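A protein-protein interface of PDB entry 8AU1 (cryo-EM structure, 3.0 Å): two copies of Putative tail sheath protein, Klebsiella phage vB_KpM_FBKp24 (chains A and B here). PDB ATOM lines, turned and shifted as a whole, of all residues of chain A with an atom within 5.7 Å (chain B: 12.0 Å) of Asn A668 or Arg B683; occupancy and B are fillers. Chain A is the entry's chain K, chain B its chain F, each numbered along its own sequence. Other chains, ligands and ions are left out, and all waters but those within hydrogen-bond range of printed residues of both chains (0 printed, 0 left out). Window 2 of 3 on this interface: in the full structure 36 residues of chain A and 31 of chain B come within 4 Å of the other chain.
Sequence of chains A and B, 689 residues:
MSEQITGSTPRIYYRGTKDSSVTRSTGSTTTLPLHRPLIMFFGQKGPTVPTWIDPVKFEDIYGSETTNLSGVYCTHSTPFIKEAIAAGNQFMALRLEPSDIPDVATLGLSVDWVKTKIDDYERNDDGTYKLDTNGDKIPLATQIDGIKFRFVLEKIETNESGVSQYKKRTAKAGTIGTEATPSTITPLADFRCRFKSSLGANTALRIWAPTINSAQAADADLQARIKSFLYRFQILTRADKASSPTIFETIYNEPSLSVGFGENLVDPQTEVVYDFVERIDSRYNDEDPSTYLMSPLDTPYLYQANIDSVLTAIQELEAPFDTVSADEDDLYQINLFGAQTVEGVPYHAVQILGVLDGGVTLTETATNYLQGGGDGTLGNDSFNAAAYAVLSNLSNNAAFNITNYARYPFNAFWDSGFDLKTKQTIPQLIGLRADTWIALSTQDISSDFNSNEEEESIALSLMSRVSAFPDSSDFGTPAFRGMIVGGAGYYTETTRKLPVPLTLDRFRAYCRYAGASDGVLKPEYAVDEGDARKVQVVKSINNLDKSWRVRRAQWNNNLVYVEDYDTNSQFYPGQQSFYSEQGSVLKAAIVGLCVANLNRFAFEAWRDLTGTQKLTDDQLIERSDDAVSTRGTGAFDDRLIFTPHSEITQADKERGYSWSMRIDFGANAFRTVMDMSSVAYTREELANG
Asn A668 touches one residue of chain B.
Printed residues of chain A within 4 Å of Arg B683: Asp A638, Arg A639, Ile A641, Ala A667 and Asn A668.
No residue of chain B comes within 4 Å of Ser A584.
Val A585 touches two residues of chain B.
No residue of chain B comes within 4 Å of Ala A588.
Of chain B, only Arg B683 (2.4 Å) comes within 4 Å of Asp A638.
Ile A641 touches just these residues of chain B: Arg B683 and Leu B686.
Gly A666 touches just these residues of chain B: Tyr B681 and Leu B686.
No residue of chain B comes within 4 Å of Ala A669.
Of the printed residues of chain B, Arg A639 touches Arg B683.
Of the printed residues of chain A, Tyr B681 touches Val A585 (3.5 Å), Gly A666 (3.1 Å) and Ala A667 (3.8 Å).
Of the printed residues of chain A, Leu B686 touches Ile A641 and Gly A666.
Of the printed residues of chain A, Thr B682 touches Val A585 (3.96 Å).
The nearest printed residue of chain A that does not touch Arg B683 is Leu A640 (4.001 Å).
No position is printed for both chains.
O of Tyr B681 touches CG2 of Val A585, 3.5 Å away.
N of Thr B682 touches CG2 of Val A585, at 3.96 Å.
O of Arg A639 touches NH1 of Arg B683, 3.8 Å away.
Arg B683 touches Ile A641 (NH2 to CG2, 3.4 Å).
Leu B686 touches Ile A641.
Gly A666 touches Tyr B681.
CD2 of Leu B686 touches N of Gly A666, 3.2 Å away.
Ala A667 touches Tyr B681 (N to O, 3.8 Å).
O of Ala A667 touches N of Arg B683 (3.7 Å).
Asn A668 touches Arg B683.
The guanidinium group (NH2) of Arg B683 is in salt-bridge range of the side-chain carboxylate (OD1) of Asp A638 (2.4 Å).
Printed residues of chain A that touch a printed residue of chain B: Val A585, Asp A638, Arg A639, Ile A641, Gly A666, Ala A667 and Asn A668.
Hydrophobic or aromatic side chains of chain B within 4 Å of the printed part of chain A: Leu B686.
Among the printed residues, 11 pairs touch across the chains.
Among the printed residues, Asp or Glu carboxylates within 4 Å of a Lys or Arg side-chain nitrogen of the other chain: Asp A638 with Arg B683 (2.4 Å).
OG1 of Thr B682 is in hydrogen-bond range of OE2 of Glu B685, 2.6 Å away.
The backbone carbonyl oxygen (O) of Ile A641 is in hydrogen-bond range of the backbone NH (N) of Gly A666.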
ATOM      1  N   SER A 584     -20.223  20.130 -13.905  1.00  0.00           N
ATOM      2  CA  SER A 584     -20.053  21.513 -14.330  1.00  0.00           C
ATOM      3  C   SER A 584     -21.031  21.932 -15.418  1.00  0.00           C
ATOM      4  O   SER A 584     -21.004  23.092 -15.838  1.00  0.00           O
ATOM      5  CB  SER A 584     -18.625  21.736 -14.828  1.00  0.00           C
ATOM      6  OG  SER A 584     -18.379  23.112 -15.044  1.00  0.00           O
ATOM      7  N   VAL A 585     -21.870  21.016 -15.904  1.00  0.00           N
ATOM      8  CA  VAL A 585     -22.888  21.381 -16.882  1.00  0.00           C
ATOM      9  C   VAL A 585     -23.982  22.210 -16.220  1.00  0.00           C
ATOM     10  O   VAL A 585     -24.464  23.198 -16.783  1.00  0.00           O
ATOM     11  CB  VAL A 585     -23.468  20.118 -17.544  1.00  0.00           C
ATOM     12  CG1 VAL A 585     -24.437  20.482 -18.650  1.00  0.00           C
ATOM     13  CG2 VAL A 585     -22.359  19.241 -18.080  1.00  0.00           C
ATOM     14  N   LYS A 587     -24.315  24.251 -13.472  1.00  0.00           N
ATOM     15  CA  LYS A 587     -23.947  25.182 -12.410  1.00  0.00           C
ATOM     16  C   LYS A 587     -24.603  26.548 -12.573  1.00  0.00           C
ATOM     17  O   LYS A 587     -25.111  27.106 -11.597  1.00  0.00           O
ATOM     18  CB  LYS A 587     -22.430  25.336 -12.347  1.00  0.00           C
ATOM     19  CG  LYS A 587     -21.693  24.071 -11.950  1.00  0.00           C
ATOM     20  CD  LYS A 587     -22.153  23.546 -10.591  1.00  0.00           C
ATOM     21  CE  LYS A 587     -21.827  24.510  -9.457  1.00  0.00           C
ATOM     22  NZ  LYS A 587     -22.290  23.986  -8.143  1.00  0.00           N
ATOM     23  N   ALA A 588     -24.598  27.110 -13.773  1.00  0.00           N
ATOM     24  CA  ALA A 588     -25.230  28.402 -13.985  1.00  0.00           C
ATOM     25  C   ALA A 588     -26.742  28.255 -13.893  1.00  0.00           C
ATOM     26  O   ALA A 588     -27.320  27.333 -14.470  1.00  0.00           O
ATOM     27  CB  ALA A 588     -24.827  28.974 -15.342  1.00  0.00           C
ATOM     28  N   VAL A 591     -29.162  28.136 -17.062  1.00  0.00           N
ATOM     29  CA  VAL A 591     -29.277  26.888 -17.806  1.00  0.00           C
ATOM     30  C   VAL A 591     -30.509  26.112 -17.360  1.00  0.00           C
ATOM     31  O   VAL A 591     -31.142  25.413 -18.159  1.00  0.00           O
ATOM     32  CB  VAL A 591     -27.991  26.061 -17.648  1.00  0.00           C
ATOM     33  CG1 VAL A 591     -28.166  24.685 -18.258  1.00  0.00           C
ATOM     34  CG2 VAL A 591     -26.825  26.794 -18.286  1.00  0.00           C
ATOM     35  N   ASP A 638     -26.818  31.173 -27.084  1.00  0.00           N
ATOM     36  CA  ASP A 638     -25.587  30.398 -26.976  1.00  0.00           C
ATOM     37  C   ASP A 638     -25.264  30.003 -25.538  1.00  0.00           C
ATOM     38  O   ASP A 638     -24.093  29.961 -25.156  1.00  0.00           O
ATOM     39  CB  ASP A 638     -24.408  31.161 -27.584  1.00  0.00           C
ATOM     40  CG  ASP A 638     -23.158  30.315 -27.689  1.00  0.00           C
ATOM     41  OD1 ASP A 638     -23.190  29.142 -27.262  1.00  0.00           O
ATOM     42  OD2 ASP A 638     -22.138  30.825 -28.198  1.00  0.00           O
ATOM     43  N   ARG A 639     -26.274  29.738 -24.712  1.00  0.00           N
ATOM     44  CA  ARG A 639     -26.011  29.158 -23.401  1.00  0.00           C
ATOM     45  C   ARG A 639     -25.976  27.636 -23.472  1.00  0.00           C
ATOM     46  O   ARG A 639     -25.307  26.989 -22.662  1.00  0.00           O
ATOM     47  CB  ARG A 639     -27.068  29.616 -22.397  1.00  0.00           C
ATOM     48  CG  ARG A 639     -27.229  31.123 -22.281  1.00  0.00           C
ATOM     49  CD  ARG A 639     -26.071  31.752 -21.539  1.00  0.00           C
ATOM     50  NE  ARG A 639     -26.327  33.143 -21.191  1.00  0.00           N
ATOM     51  CZ  ARG A 639     -25.567  33.862 -20.377  1.00  0.00           C
ATOM     52  NH1 ARG A 639     -24.491  33.352 -19.807  1.00  0.00           N
ATOM     53  NH2 ARG A 639     -25.896  35.125 -20.129  1.00  0.00           N
ATOM     54  N   LEU A 640     -26.688  27.055 -24.434  1.00  0.00           N
ATOM     55  CA  LEU A 640     -26.813  25.617 -24.598  1.00  0.00           C
ATOM     56  C   LEU A 640     -26.471  25.215 -26.023  1.00  0.00           C
ATOM     57  O   LEU A 640     -26.480  26.037 -26.941  1.00  0.00           O
ATOM     58  CB  LEU A 640     -28.241  25.142 -24.313  1.00  0.00           C
ATOM     59  CG  LEU A 640     -28.756  25.030 -22.886  1.00  0.00           C
ATOM     60  CD1 LEU A 640     -30.105  24.353 -22.903  1.00  0.00           C
ATOM     61  CD2 LEU A 640     -27.791  24.266 -22.027  1.00  0.00           C
ATOM     62  N   ILE A 641     -26.183  23.929 -26.204  1.00  0.00           N
ATOM     63  CA  ILE A 641     -26.305  23.291 -27.512  1.00  0.00           C
ATOM     64  C   ILE A 641     -27.057  21.984 -27.319  1.00  0.00           C
ATOM     65  O   ILE A 641     -26.682  21.174 -26.470  1.00  0.00           O
ATOM     66  CB  ILE A 641     -24.942  23.054 -28.186  1.00  0.00           C
ATOM     67  CG1 ILE A 641     -24.032  22.213 -27.298  1.00  0.00           C
ATOM     68  CG2 ILE A 641     -24.282  24.375 -28.497  1.00  0.00           C
ATOM     69  CD1 ILE A 641     -22.672  21.982 -27.887  1.00  0.00           C
ATOM     70  N   GLY A 666     -25.821  20.373 -23.834  1.00  0.00           N
ATOM     71  CA  GLY A 666     -24.521  20.629 -23.237  1.00  0.00           C
ATOM     72  C   GLY A 666     -24.300  22.104 -22.990  1.00  0.00           C
ATOM     73  O   GLY A 666     -24.742  22.957 -23.768  1.00  0.00           O
ATOM     74  N   ALA A 667     -23.576  22.399 -21.903  1.00  0.00           N
ATOM     75  CA  ALA A 667     -23.374  23.754 -21.404  1.00  0.00           C
ATOM     76  C   ALA A 667     -21.997  23.852 -20.754  1.00  0.00           C
ATOM     77  O   ALA A 667     -21.262  22.869 -20.668  1.00  0.00           O
ATOM     78  CB  ALA A 667     -24.462  24.138 -20.405  1.00  0.00           C
ATOM     79  N   ASN A 668     -21.658  25.058 -20.291  1.00  0.00           N
ATOM     80  CA  ASN A 668     -20.364  25.373 -19.689  1.00  0.00           C
ATOM     81  C   ASN A 668     -20.540  25.935 -18.278  1.00  0.00           C
ATOM     82  O   ASN A 668     -21.649  26.044 -17.754  1.00  0.00           O
ATOM     83  CB  ASN A 668     -19.593  26.379 -20.547  1.00  0.00           C
ATOM     84  CG  ASN A 668     -18.770  25.722 -21.621  1.00  0.00           C
ATOM     85  OD1 ASN A 668     -18.215  24.645 -21.420  1.00  0.00           O
ATOM     86  ND2 ASN A 668     -18.661  26.379 -22.766  1.00  0.00           N
ATOM     87  N   ALA A 669     -19.407  26.299 -17.668  1.00  0.00           N
ATOM     88  CA  ALA A 669     -19.373  26.963 -16.369  1.00  0.00           C
ATOM     89  C   ALA A 669     -18.418  28.151 -16.418  1.00  0.00           C
ATOM     90  O   ALA A 669     -17.975  28.545 -17.500  1.00  0.00           O
ATOM     91  CB  ALA A 669     -18.954  25.988 -15.271  1.00  0.00           C
ATOM     92  N   PHE A 670     -18.087  28.723 -15.261  1.00  0.00           N
ATOM     93  CA  PHE A 670     -17.284  29.935 -15.183  1.00  0.00           C
ATOM     94  C   PHE A 670     -16.165  29.781 -14.163  1.00  0.00           C
ATOM     95  O   PHE A 670     -16.239  28.950 -13.256  1.00  0.00           O
ATOM     96  CB  PHE A 670     -18.149  31.135 -14.814  1.00  0.00           C
ATOM     97  CG  PHE A 670     -19.119  30.862 -13.701  1.00  0.00           C
ATOM     98  CD1 PHE A 670     -20.444  30.596 -13.975  1.00  0.00           C
ATOM     99  CD2 PHE A 670     -18.708  30.866 -12.385  1.00  0.00           C
ATOM    100  CE1 PHE A 670     -21.335  30.347 -12.963  1.00  0.00           C
ATOM    101  CE2 PHE A 670     -19.600  30.614 -11.371  1.00  0.00           C
ATOM    102  CZ  PHE A 670     -20.914  30.351 -11.663  1.00  0.00           C
ATOM    103  N   VAL B 679     -30.186  13.855 -21.297  1.00  0.00           N
ATOM    104  CA  VAL B 679     -28.878  13.534 -20.748  1.00  0.00           C
ATOM    105  C   VAL B 679     -28.023  14.788 -20.810  1.00  0.00           C
ATOM    106  O   VAL B 679     -28.084  15.544 -21.782  1.00  0.00           O
ATOM    107  CB  VAL B 679     -28.206  12.371 -21.498  1.00  0.00           C
ATOM    108  CG1 VAL B 679     -29.014  11.108 -21.335  1.00  0.00           C
ATOM    109  CG2 VAL B 679     -28.063  12.705 -22.941  1.00  0.00           C
ATOM    110  N   ALA B 680     -27.235  15.011 -19.766  1.00  0.00           N
ATOM    111  CA  ALA B 680     -26.389  16.188 -19.660  1.00  0.00           C
ATOM    112  C   ALA B 680     -24.977  15.832 -20.095  1.00  0.00           C
ATOM    113  O   ALA B 680     -24.334  14.973 -19.487  1.00  0.00           O
ATOM    114  CB  ALA B 680     -26.382  16.723 -18.231  1.00  0.00           C
ATOM    115  N   TYR B 681     -24.503  16.495 -21.138  1.00  0.00           N
ATOM    116  CA  TYR B 681     -23.160  16.305 -21.654  1.00  0.00           C
ATOM    117  C   TYR B 681     -22.370  17.588 -21.473  1.00  0.00           C
ATOM    118  O   TYR B 681     -22.932  18.683 -21.437  1.00  0.00           O
ATOM    119  CB  TYR B 681     -23.177  15.939 -23.139  1.00  0.00           C
ATOM    120  CG  TYR B 681     -23.598  14.528 -23.440  1.00  0.00           C
ATOM    121  CD1 TYR B 681     -22.820  13.456 -23.047  1.00  0.00           C
ATOM    122  CD2 TYR B 681     -24.767  14.269 -24.130  1.00  0.00           C
ATOM    123  CE1 TYR B 681     -23.196  12.169 -23.326  1.00  0.00           C
ATOM    124  CE2 TYR B 681     -25.150  12.985 -24.415  1.00  0.00           C
ATOM    125  CZ  TYR B 681     -24.359  11.937 -24.012  1.00  0.00           C
ATOM    126  OH  TYR B 681     -24.738  10.648 -24.292  1.00  0.00           O
ATOM    127  N   THR B 682     -21.055  17.455 -21.362  1.00  0.00           N
ATOM    128  CA  THR B 682     -20.228  18.639 -21.463  1.00  0.00           C
ATOM    129  C   THR B 682     -20.176  19.095 -22.916  1.00  0.00           C
ATOM    130  O   THR B 682     -20.391  18.319 -23.854  1.00  0.00           O
ATOM    131  CB  THR B 682     -18.818  18.383 -20.935  1.00  0.00           C
ATOM    132  OG1 THR B 682     -18.124  17.494 -21.814  1.00  0.00           O
ATOM    133  CG2 THR B 682     -18.870  17.772 -19.552  1.00  0.00           C
ATOM    134  N   ARG B 683     -19.886  20.381 -23.094  1.00  0.00           N
ATOM    135  CA  ARG B 683     -19.997  20.978 -24.418  1.00  0.00           C
ATOM    136  C   ARG B 683     -19.080  20.285 -25.413  1.00  0.00           C
ATOM    137  O   ARG B 683     -19.469  20.047 -26.560  1.00  0.00           O
ATOM    138  CB  ARG B 683     -19.678  22.465 -24.342  1.00  0.00           C
ATOM    139  CG  ARG B 683     -20.608  23.311 -25.165  1.00  0.00           C
ATOM    140  CD  ARG B 683     -20.018  24.668 -25.433  1.00  0.00           C
ATOM    141  NE  ARG B 683     -20.842  25.431 -26.360  1.00  0.00           N
ATOM    142  CZ  ARG B 683     -21.883  26.165 -26.001  1.00  0.00           C
ATOM    143  NH1 ARG B 683     -22.264  26.251 -24.737  1.00  0.00           N
ATOM    144  NH2 ARG B 683     -22.558  26.830 -26.931  1.00  0.00           N
ATOM    145  N   GLU B 684     -17.861  19.945 -24.997  1.00  0.00           N
ATOM    146  CA  GLU B 684     -16.905  19.369 -25.935  1.00  0.00           C
ATOM    147  C   GLU B 684     -17.314  17.968 -26.365  1.00  0.00           C
ATOM    148  O   GLU B 684     -17.298  17.655 -27.561  1.00  0.00           O
ATOM    149  CB  GLU B 684     -15.511  19.350 -25.314  1.00  0.00           C
ATOM    150  CG  GLU B 684     -14.948  20.736 -25.078  1.00  0.00           C
ATOM    151  CD  GLU B 684     -14.681  21.478 -26.371  1.00  0.00           C
ATOM    152  OE1 GLU B 684     -14.349  20.819 -27.377  1.00  0.00           O
ATOM    153  OE2 GLU B 684     -14.816  22.719 -26.385  1.00  0.00           O
ATOM    154  N   GLU B 685     -17.680  17.108 -25.416  1.00  0.00           N
ATOM    155  CA  GLU B 685     -18.047  15.750 -25.790  1.00  0.00           C
ATOM    156  C   GLU B 685     -19.402  15.686 -26.471  1.00  0.00           C
ATOM    157  O   GLU B 685     -19.704  14.672 -27.104  1.00  0.00           O
ATOM    158  CB  GLU B 685     -18.037  14.828 -24.570  1.00  0.00           C
ATOM    159  CG  GLU B 685     -19.079  15.142 -23.527  1.00  0.00           C
ATOM    160  CD  GLU B 685     -18.851  14.372 -22.238  1.00  0.00           C
ATOM    161  OE1 GLU B 685     -18.999  13.132 -22.250  1.00  0.00           O
ATOM    162  OE2 GLU B 685     -18.522  15.002 -21.211  1.00  0.00           O
ATOM    163  N   LEU B 686     -20.222  16.728 -26.359  1.00  0.00           N
ATOM    164  CA  LEU B 686     -21.441  16.800 -27.152  1.00  0.00           C
ATOM    165  C   LEU B 686     -21.200  17.348 -28.548  1.00  0.00           C
ATOM    166  O   LEU B 686     -21.872  16.925 -29.492  1.00  0.00           O
ATOM    167  CB  LEU B 686     -22.485  17.669 -26.446  1.00  0.00           C
ATOM    168  CG  LEU B 686     -23.786  17.914 -27.204  1.00  0.00           C
ATOM    169  CD1 LEU B 686     -24.434  16.607 -27.596  1.00  0.00           C
ATOM    170  CD2 LEU B 686     -24.725  18.712 -26.341  1.00  0.00           C
ATOM    171  N   ALA B 687     -20.255  18.276 -28.700  1.00  0.00           N
ATOM    172  CA  ALA B 687     -19.951  18.830 -30.011  1.00  0.00           C
ATOM    173  C   ALA B 687     -19.128  17.875 -30.862  1.00  0.00           C
ATOM    174  O   ALA B 687     -19.239  17.901 -32.092  1.00  0.00           O
ATOM    175  CB  ALA B 687     -19.204  20.155 -29.854  1.00  0.00           C
ATOM    176  N   ASN B 688     -18.301  17.040 -30.241  1.00  0.00           N
ATOM    177  CA  ASN B 688     -17.416  16.156 -30.993  1.00  0.00           C
ATOM    178  C   ASN B 688     -16.981  15.007 -30.099  1.00  0.00           C
ATOM    179  O   ASN B 688     -16.251  15.221 -29.128  1.00  0.00           O
ATOM    180  CB  ASN B 688     -16.206  16.929 -31.504  1.00  0.00           C
ATOM    181  CG  ASN B 688     -15.509  17.701 -30.405  1.00  0.00           C
ATOM    182  OD1 ASN B 688     -14.637  17.175 -29.717  1.00  0.00           O
ATOM    183  ND2 ASN B 688     -15.902  18.957 -30.226  1.00  0.00           N
ATOM    184  N   GLY B 689     -17.416  13.796 -30.432  1.00  0.00           N
ATOM    185  CA  GLY B 689     -17.036  12.615 -29.679  1.00  0.00           C
ATOM    186  C   GLY B 689     -18.019  12.267 -28.579  1.00  0.00           C
ATOM    187  O   GLY B 689     -18.817  11.340 -28.718  1.00  0.00           O
